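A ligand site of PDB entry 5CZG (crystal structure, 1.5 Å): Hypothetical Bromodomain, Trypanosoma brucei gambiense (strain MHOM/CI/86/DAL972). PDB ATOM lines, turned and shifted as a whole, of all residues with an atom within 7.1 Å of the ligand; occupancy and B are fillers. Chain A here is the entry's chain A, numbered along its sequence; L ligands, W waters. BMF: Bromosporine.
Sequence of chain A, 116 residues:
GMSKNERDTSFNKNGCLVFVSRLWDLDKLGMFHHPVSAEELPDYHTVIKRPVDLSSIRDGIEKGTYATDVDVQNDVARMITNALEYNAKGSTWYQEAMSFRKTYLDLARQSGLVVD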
ATOM      1  N   GLY A  30     -21.343 -13.051 -24.105  1.00  0.00           N
ATOM      2  CA  GLY A  30     -20.627 -12.500 -22.966  1.00  0.00           C
ATOM      3  C   GLY A  30     -21.572 -11.812 -21.993  1.00  0.00           C
ATOM      4  O   GLY A  30     -21.149 -10.954 -21.217  1.00  0.00           O
ATOM      5  N   MET A  31     -22.846 -12.193 -22.027  1.00  0.00           N
ATOM      6  CA  MET A  31     -23.860 -11.455 -21.259  1.00  0.00           C
ATOM      7  C   MET A  31     -23.753 -11.687 -19.748  1.00  0.00           C
ATOM      8  O   MET A  31     -24.156 -10.812 -18.980  1.00  0.00           O
ATOM      9  CB  MET A  31     -25.279 -11.759 -21.753  1.00  0.00           C
ATOM     10  CG  MET A  31     -25.816 -13.143 -21.433  1.00  0.00           C
ATOM     11  SD  MET A  31     -27.545 -13.354 -21.926  1.00  0.00           S
ATOM     12  CE  MET A  31     -28.458 -12.605 -20.594  1.00  0.00           C
ATOM     13  N   PHE A  32     -23.217 -12.845 -19.348  1.00  0.00           N
ATOM     14  CA  PHE A  32     -23.071 -13.214 -17.946  1.00  0.00           C
ATOM     15  C   PHE A  32     -21.655 -13.016 -17.422  1.00  0.00           C
ATOM     16  O   PHE A  32     -21.370 -13.300 -16.255  1.00  0.00           O
ATOM     17  CB  PHE A  32     -23.472 -14.683 -17.750  1.00  0.00           C
ATOM     18  CG  PHE A  32     -24.923 -14.972 -18.033  1.00  0.00           C
ATOM     19  CD1 PHE A  32     -25.918 -14.395 -17.276  1.00  0.00           C
ATOM     20  CD2 PHE A  32     -25.277 -15.856 -19.036  1.00  0.00           C
ATOM     21  CE1 PHE A  32     -27.255 -14.688 -17.516  1.00  0.00           C
ATOM     22  CE2 PHE A  32     -26.606 -16.153 -19.281  1.00  0.00           C
ATOM     23  CZ  PHE A  32     -27.597 -15.563 -18.530  1.00  0.00           C
ATOM     24  N   HIS A  33     -20.746 -12.550 -18.264  1.00  0.00           N
ATOM     25  CA  HIS A  33     -19.337 -12.422 -17.880  1.00  0.00           C
ATOM     26  C   HIS A  33     -19.111 -11.427 -16.763  1.00  0.00           C
ATOM     27  O   HIS A  33     -18.319 -11.691 -15.851  1.00  0.00           O
ATOM     28  CB  HIS A  33     -18.499 -12.009 -19.091  1.00  0.00           C
ATOM     29  CG  HIS A  33     -18.258 -13.113 -20.065  1.00  0.00           C
ATOM     30  ND1 HIS A  33     -17.470 -12.962 -21.177  1.00  0.00           N
ATOM     31  CD2 HIS A  33     -18.700 -14.396 -20.090  1.00  0.00           C
ATOM     32  CE1 HIS A  33     -17.441 -14.088 -21.858  1.00  0.00           C
ATOM     33  NE2 HIS A  33     -18.180 -14.977 -21.219  1.00  0.00           N
ATOM     34  N   HIS A  34     -19.782 -10.279 -16.821  1.00  0.00           N
ATOM     35  CA  HIS A  34     -19.550  -9.174 -15.902  1.00  0.00           C
ATOM     36  C   HIS A  34     -20.866  -8.676 -15.324  1.00  0.00           C
ATOM     37  O   HIS A  34     -21.925  -8.964 -15.883  1.00  0.00           O
ATOM     38  CB  HIS A  34     -18.811  -8.052 -16.633  1.00  0.00           C
ATOM     39  CG  HIS A  34     -17.499  -8.485 -17.192  1.00  0.00           C
ATOM     40  ND1 HIS A  34     -16.405  -8.758 -16.395  1.00  0.00           N
ATOM     41  CD2 HIS A  34     -17.119  -8.721 -18.467  1.00  0.00           C
ATOM     42  CE1 HIS A  34     -15.401  -9.144 -17.165  1.00  0.00           C
ATOM     43  NE2 HIS A  34     -15.805  -9.135 -18.420  1.00  0.00           N
ATOM     44  N   PRO A  35     -20.801  -7.970 -14.183  1.00  0.00           N
ATOM     45  CA  PRO A  35     -22.046  -7.497 -13.591  1.00  0.00           C
ATOM     46  C   PRO A  35     -22.822  -6.610 -14.544  1.00  0.00           C
ATOM     47  O   PRO A  35     -22.246  -5.861 -15.366  1.00  0.00           O
ATOM     48  CB  PRO A  35     -21.570  -6.654 -12.413  1.00  0.00           C
ATOM     49  CG  PRO A  35     -20.214  -7.158 -12.082  1.00  0.00           C
ATOM     50  CD  PRO A  35     -19.623  -7.581 -13.394  1.00  0.00           C
ATOM     51  N   VAL A  36     -24.148  -6.686 -14.454  1.00  0.00           N
ATOM     52  CA  VAL A  36     -24.982  -5.694 -15.130  1.00  0.00           C
ATOM     53  C   VAL A  36     -24.665  -4.324 -14.534  1.00  0.00           C
ATOM     54  O   VAL A  36     -24.714  -4.107 -13.315  1.00  0.00           O
ATOM     55  CB  VAL A  36     -26.482  -5.989 -14.993  1.00  0.00           C
ATOM     56  CG1 VAL A  36     -27.291  -4.792 -15.497  1.00  0.00           C
ATOM     57  CG2 VAL A  36     -26.839  -7.246 -15.738  1.00  0.00           C
ATOM     58  N   SER A  37     -24.323  -3.396 -15.416  1.00  0.00           N
ATOM     59  CA  SER A  37     -24.006  -2.038 -15.045  1.00  0.00           C
ATOM     60  C   SER A  37     -25.281  -1.197 -15.106  1.00  0.00           C
ATOM     61  O   SER A  37     -26.025  -1.261 -16.083  1.00  0.00           O
ATOM     62  CB  SER A  37     -22.976  -1.497 -16.038  1.00  0.00           C
ATOM     63  OG  SER A  37     -22.876  -0.092 -15.985  1.00  0.00           O
ATOM     64  N   GLU A  40     -25.633   0.869 -18.133  1.00  0.00           N
ATOM     65  CA  GLU A  40     -26.102   0.192 -19.328  1.00  0.00           C
ATOM     66  C   GLU A  40     -27.593  -0.132 -19.236  1.00  0.00           C
ATOM     67  O   GLU A  40     -28.315   0.009 -20.219  1.00  0.00           O
ATOM     68  CB  GLU A  40     -25.292  -1.081 -19.589  1.00  0.00           C
ATOM     69  CG  GLU A  40     -23.776  -0.905 -19.673  1.00  0.00           C
ATOM     70  CD  GLU A  40     -23.327  -0.181 -20.917  1.00  0.00           C
ATOM     71  OE1 GLU A  40     -24.149   0.024 -21.824  1.00  0.00           O
ATOM     72  OE2 GLU A  40     -22.124   0.171 -20.995  1.00  0.00           O
ATOM     73  N   LEU A  41     -28.065  -0.544 -18.064  1.00  0.00           N
ATOM     74  CA  LEU A  41     -29.480  -0.861 -17.852  1.00  0.00           C
ATOM     75  C   LEU A  41     -29.980  -0.167 -16.582  1.00  0.00           C
ATOM     76  O   LEU A  41     -30.013  -0.770 -15.494  1.00  0.00           O
ATOM     77  CB  LEU A  41     -29.706  -2.372 -17.737  1.00  0.00           C
ATOM     78  CG  LEU A  41     -29.433  -3.216 -18.987  1.00  0.00           C
ATOM     79  CD1 LEU A  41     -29.638  -4.688 -18.658  1.00  0.00           C
ATOM     80  CD2 LEU A  41     -30.309  -2.769 -20.186  1.00  0.00           C
ATOM     81  N   ASP A  43     -32.840   0.596 -15.498  1.00  0.00           N
ATOM     82  CA  ASP A  43     -34.091   0.110 -14.901  1.00  0.00           C
ATOM     83  C   ASP A  43     -33.965  -1.328 -14.399  1.00  0.00           C
ATOM     84  O   ASP A  43     -34.951  -1.946 -14.035  1.00  0.00           O
ATOM     85  CB  ASP A  43     -35.284   0.251 -15.867  1.00  0.00           C
ATOM     86  CG  ASP A  43     -35.287  -0.767 -16.981  1.00  0.00           C
ATOM     87  OD1 ASP A  43     -34.233  -1.408 -17.235  1.00  0.00           O
ATOM     88  OD2 ASP A  43     -36.365  -0.912 -17.638  1.00  0.00           O
ATOM     89  N   TYR A  44     -32.750  -1.853 -14.412  1.00  0.00           N
ATOM     90  CA  TYR A  44     -32.529  -3.257 -14.044  1.00  0.00           C
ATOM     91  C   TYR A  44     -32.679  -3.557 -12.551  1.00  0.00           C
ATOM     92  O   TYR A  44     -33.355  -4.503 -12.183  1.00  0.00           O
ATOM     93  CB  TYR A  44     -31.159  -3.688 -14.531  1.00  0.00           C
ATOM     94  CG  TYR A  44     -30.796  -5.140 -14.290  1.00  0.00           C
ATOM     95  CD1 TYR A  44     -31.196  -6.132 -15.182  1.00  0.00           C
ATOM     96  CD2 TYR A  44     -30.023  -5.528 -13.186  1.00  0.00           C
ATOM     97  CE1 TYR A  44     -30.854  -7.466 -14.981  1.00  0.00           C
ATOM     98  CE2 TYR A  44     -29.672  -6.849 -13.003  1.00  0.00           C
ATOM     99  CZ  TYR A  44     -30.093  -7.809 -13.894  1.00  0.00           C
ATOM    100  OH  TYR A  44     -29.757  -9.115 -13.685  1.00  0.00           O
ATOM    101  N   VAL A  52     -25.995 -11.093  -9.911  1.00  0.00           N
ATOM    102  CA  VAL A  52     -24.783 -11.864  -9.826  1.00  0.00           C
ATOM    103  C   VAL A  52     -24.318 -12.191 -11.240  1.00  0.00           C
ATOM    104  O   VAL A  52     -25.116 -12.183 -12.182  1.00  0.00           O
ATOM    105  CB  VAL A  52     -24.999 -13.107  -8.935  1.00  0.00           C
ATOM    106  CG1 VAL A  52     -26.032 -14.022  -9.551  1.00  0.00           C
ATOM    107  CG2 VAL A  52     -23.701 -13.833  -8.708  1.00  0.00           C
ATOM    108  N   MET A  79     -28.513 -16.276 -11.222  1.00  0.00           N
ATOM    109  CA  MET A  79     -28.044 -15.492 -12.361  1.00  0.00           C
ATOM    110  C   MET A  79     -28.956 -15.691 -13.553  1.00  0.00           C
ATOM    111  O   MET A  79     -29.342 -14.732 -14.251  1.00  0.00           O
ATOM    112  CB  MET A  79     -26.609 -15.947 -12.697  1.00  0.00           C
ATOM    113  CG  MET A  79     -25.937 -15.136 -13.782  1.00  0.00           C
ATOM    114  SD  MET A  79     -24.314 -15.765 -14.202  1.00  0.00           S
ATOM    115  CE  MET A  79     -24.744 -17.243 -15.120  1.00  0.00           C
ATOM    116  N   ASN A  82     -32.592 -14.430 -12.822  1.00  0.00           N
ATOM    117  CA  ASN A  82     -32.628 -12.963 -12.902  1.00  0.00           C
ATOM    118  C   ASN A  82     -32.829 -12.530 -14.346  1.00  0.00           C
ATOM    119  O   ASN A  82     -33.632 -11.635 -14.644  1.00  0.00           O
ATOM    120  CB  ASN A  82     -31.306 -12.356 -12.444  1.00  0.00           C
ATOM    121  CG  ASN A  82     -31.119 -12.382 -10.930  1.00  0.00           C
ATOM    122  OD1 ASN A  82     -32.065 -12.586 -10.177  1.00  0.00           O
ATOM    123  ND2 ASN A  82     -29.888 -12.114 -10.497  1.00  0.00           N
ATOM    124  N   ALA A  83     -32.106 -13.169 -15.259  1.00  0.00           N
ATOM    125  CA  ALA A  83     -32.223 -12.807 -16.671  1.00  0.00           C
ATOM    126  C   ALA A  83     -33.618 -13.119 -17.225  1.00  0.00           C
ATOM    127  O   ALA A  83     -34.157 -12.355 -18.036  1.00  0.00           O
ATOM    128  CB  ALA A  83     -31.165 -13.507 -17.486  1.00  0.00           C
ATOM    129  N   LEU A  84     -34.204 -14.228 -16.813  1.00  0.00           N
ATOM    130  CA  LEU A  84     -35.533 -14.594 -17.273  1.00  0.00           C
ATOM    131  C   LEU A  84     -36.663 -13.800 -16.599  1.00  0.00           C
ATOM    132  O   LEU A  84     -37.760 -13.700 -17.154  1.00  0.00           O
ATOM    133  CB  LEU A  84     -35.746 -16.096 -17.143  1.00  0.00           C
ATOM    134  CG  LEU A  84     -34.836 -16.948 -18.019  1.00  0.00           C
ATOM    135  CD1 LEU A  84     -34.926 -18.418 -17.631  1.00  0.00           C
ATOM    136  CD2 LEU A  84     -35.151 -16.748 -19.499  1.00  0.00           C
ATOM    137  N   TYR A  86     -36.125 -10.422 -15.712  1.00  0.00           N
ATOM    138  CA  TYR A  86     -35.988  -9.076 -16.252  1.00  0.00           C
ATOM    139  C   TYR A  86     -36.387  -8.988 -17.724  1.00  0.00           C
ATOM    140  O   TYR A  86     -37.080  -8.053 -18.132  1.00  0.00           O
ATOM    141  CB  TYR A  86     -34.550  -8.568 -16.067  1.00  0.00           C
ATOM    142  CG  TYR A  86     -34.335  -7.237 -16.720  1.00  0.00           C
ATOM    143  CD1 TYR A  86     -34.789  -6.068 -16.115  1.00  0.00           C
ATOM    144  CD2 TYR A  86     -33.701  -7.140 -17.951  1.00  0.00           C
ATOM    145  CE1 TYR A  86     -34.602  -4.825 -16.732  1.00  0.00           C
ATOM    146  CE2 TYR A  86     -33.511  -5.914 -18.568  1.00  0.00           C
ATOM    147  CZ  TYR A  86     -33.954  -4.755 -17.960  1.00  0.00           C
ATOM    148  OH  TYR A  86     -33.763  -3.547 -18.601  1.00  0.00           O
ATOM    149  N   ASN A  87     -35.931  -9.953 -18.514  1.00  0.00           N
ATOM    150  CA  ASN A  87     -36.044  -9.844 -19.982  1.00  0.00           C
ATOM    151  C   ASN A  87     -37.411 -10.251 -20.530  1.00  0.00           C
ATOM    152  O   ASN A  87     -38.193 -10.917 -19.847  1.00  0.00           O
ATOM    153  CB  ASN A  87     -34.918 -10.645 -20.634  1.00  0.00           C
ATOM    154  CG  ASN A  87     -33.576  -9.975 -20.481  1.00  0.00           C
ATOM    155  OD1 ASN A  87     -33.293  -8.954 -21.118  1.00  0.00           O
ATOM    156  ND2 ASN A  87     -32.729 -10.524 -19.619  1.00  0.00           N
ATOM    157  N   ALA A  88     -37.679  -9.834 -21.750  1.00  0.00           N
ATOM    158  CA  ALA A  88     -38.942 -10.114 -22.437  1.00  0.00           C
ATOM    159  C   ALA A  88     -38.787 -11.358 -23.273  1.00  0.00           C
ATOM    160  O   ALA A  88     -37.812 -11.467 -24.027  1.00  0.00           O
ATOM    161  CB  ALA A  88     -39.325  -8.946 -23.304  1.00  0.00           C
ATOM    162  N   SER A  91     -36.483 -12.139 -26.696  1.00  0.00           N
ATOM    163  CA  SER A  91     -35.287 -11.314 -26.929  1.00  0.00           C
ATOM    164  C   SER A  91     -34.040 -12.181 -26.975  1.00  0.00           C
ATOM    165  O   SER A  91     -34.047 -13.337 -26.551  1.00  0.00           O
ATOM    166  CB  SER A  91     -35.105 -10.258 -25.834  1.00  0.00           C
ATOM    167  OG  SER A  91     -34.662 -10.856 -24.628  1.00  0.00           O
ATOM    168  N   TRP A  93     -31.374 -11.888 -25.225  1.00  0.00           N
ATOM    169  CA  TRP A  93     -30.924 -12.163 -23.860  1.00  0.00           C
ATOM    170  C   TRP A  93     -31.762 -13.280 -23.235  1.00  0.00           C
ATOM    171  O   TRP A  93     -31.241 -14.186 -22.536  1.00  0.00           O
ATOM    172  CB  TRP A  93     -31.007 -10.880 -23.029  1.00  0.00           C
ATOM    173  CG  TRP A  93     -30.540  -9.650 -23.772  1.00  0.00           C
ATOM    174  CD1 TRP A  93     -31.315  -8.678 -24.330  1.00  0.00           C
ATOM    175  CD2 TRP A  93     -29.184  -9.288 -24.037  1.00  0.00           C
ATOM    176  NE1 TRP A  93     -30.532  -7.725 -24.914  1.00  0.00           N
ATOM    177  CE2 TRP A  93     -29.213  -8.070 -24.752  1.00  0.00           C
ATOM    178  CE3 TRP A  93     -27.950  -9.855 -23.741  1.00  0.00           C
ATOM    179  CZ2 TRP A  93     -28.061  -7.413 -25.178  1.00  0.00           C
ATOM    180  CZ3 TRP A  93     -26.803  -9.199 -24.155  1.00  0.00           C
ATOM    181  CH2 TRP A  93     -26.864  -7.999 -24.862  1.00  0.00           C
ATOM    182  N   TYR A  94     -33.073 -13.242 -23.463  1.00  0.00           N
ATOM    183  CA  TYR A  94     -33.972 -14.268 -22.959  1.00  0.00           C
ATOM    184  C   TYR A  94     -33.592 -15.629 -23.548  1.00  0.00           C
ATOM    185  O   TYR A  94     -33.551 -16.626 -22.828  1.00  0.00           O
ATOM    186  CB  TYR A  94     -35.444 -13.924 -23.267  1.00  0.00           C
ATOM    187  CG  TYR A  94     -36.397 -15.110 -23.325  1.00  0.00           C
ATOM    188  CD1 TYR A  94     -36.527 -15.861 -24.491  1.00  0.00           C
ATOM    189  CD2 TYR A  94     -37.199 -15.453 -22.248  1.00  0.00           C
ATOM    190  CE1 TYR A  94     -37.414 -16.928 -24.573  1.00  0.00           C
ATOM    191  CE2 TYR A  94     -38.075 -16.523 -22.310  1.00  0.00           C
ATOM    192  CZ  TYR A  94     -38.182 -17.252 -23.480  1.00  0.00           C
ATOM    193  OH  TYR A  94     -39.053 -18.320 -23.555  1.00  0.00           O
ATOM    194  N   ALA A  97     -30.479 -17.010 -21.962  1.00  0.00           N
ATOM    195  CA  ALA A  97     -30.748 -17.427 -20.601  1.00  0.00           C
ATOM    196  C   ALA A  97     -31.510 -18.760 -20.593  1.00  0.00           C
ATOM    197  O   ALA A  97     -31.261 -19.609 -19.730  1.00  0.00           O
ATOM    198  CB  ALA A  97     -31.506 -16.350 -19.835  1.00  0.00           C
HETATM  199  C10 BMF L   1     -26.038  -6.359 -21.790  1.00  0.00           C
HETATM  200  N12 BMF L   1     -27.047  -7.928 -20.188  1.00  0.00           N
HETATM  201  C15 BMF L   1     -29.743  -7.381 -21.077  1.00  0.00           C
HETATM  202  C17 BMF L   1     -31.535  -6.091 -22.240  1.00  0.00           C
HETATM  203  C20 BMF L   1     -33.830  -3.950 -21.984  1.00  0.00           C
HETATM  204  C22 BMF L   1     -28.651  -6.740 -21.632  1.00  0.00           C
HETATM  205  C26 BMF L   1     -26.964  -9.958 -17.982  1.00  0.00           C
HETATM  206  C09 BMF L   1     -25.229  -5.460 -21.057  1.00  0.00           C
HETATM  207  C11 BMF L   1     -27.278  -7.031 -21.194  1.00  0.00           C
HETATM  208  N13 BMF L   1     -28.180  -8.532 -19.671  1.00  0.00           N
HETATM  209  C14 BMF L   1     -29.511  -8.294 -20.033  1.00  0.00           C
HETATM  210  N16 BMF L   1     -31.103  -7.167 -21.423  1.00  0.00           N
HETATM  211  O18 BMF L   1     -32.899  -6.186 -22.347  1.00  0.00           O
HETATM  212  C19 BMF L   1     -33.462  -5.028 -23.008  1.00  0.00           C
HETATM  213  O21 BMF L   1     -30.802  -5.288 -22.703  1.00  0.00           O
HETATM  214  N23 BMF L   1     -30.295  -9.071 -19.251  1.00  0.00           N
HETATM  215  N24 BMF L   1     -29.471  -9.791 -18.396  1.00  0.00           N
HETATM  216  C25 BMF L   1     -28.194  -9.480 -18.615  1.00  0.00           C
HETATM  217  O   HOH W   1     -24.335  -9.981 -16.317  1.00  0.00           O
HETATM  218  O   HOH W   2     -30.034 -10.690 -15.697  1.00  0.00           O
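Water W2 lies within hydrogen-bond range of the side-chain hydroxyl of Tyr 44 (2.6 Å), a nitrogen (N24) of the ligand (2.9 Å) and the backbone NH of Ala 83 (3.3 Å).
Residues that only touch the ligand: Met 31 (3.1 Å), Val 36 (3.5 Å), Leu 41 (3.6 Å) and Tyr 86 (3.4 Å). Within 4 Å of the ligand: Met 31, Val 36, Leu 41, Tyr 86, Asn 87 and Trp 93. Along chain A the residues within 4 Å of the ligand span positions 31 to 93.
The backbone carbonyl oxygen (O) of Ala 83 is in hydrogen-bond range of the side-chain amide nitrogen (ND2) of Asn 87 (2.8 Å). The side-chain hydroxyl (OG) of Ser 91 sits close to the backbone NH (N) of Trp 93 (3.5 Å). The side-chain hydroxyl (OH) of Tyr 86 sits at hydrogen-bond distance from the side-chain carboxylate (OD1) of Asp 43 (2.6 Å).
The side-chain amide oxygen of Asn 87 is in hydrogen-bond range of a nitrogen (N16) of the ligand (2.8 Å). NE1 of Trp 93 sits close to O21 of the ligand, at 3.3 Å.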
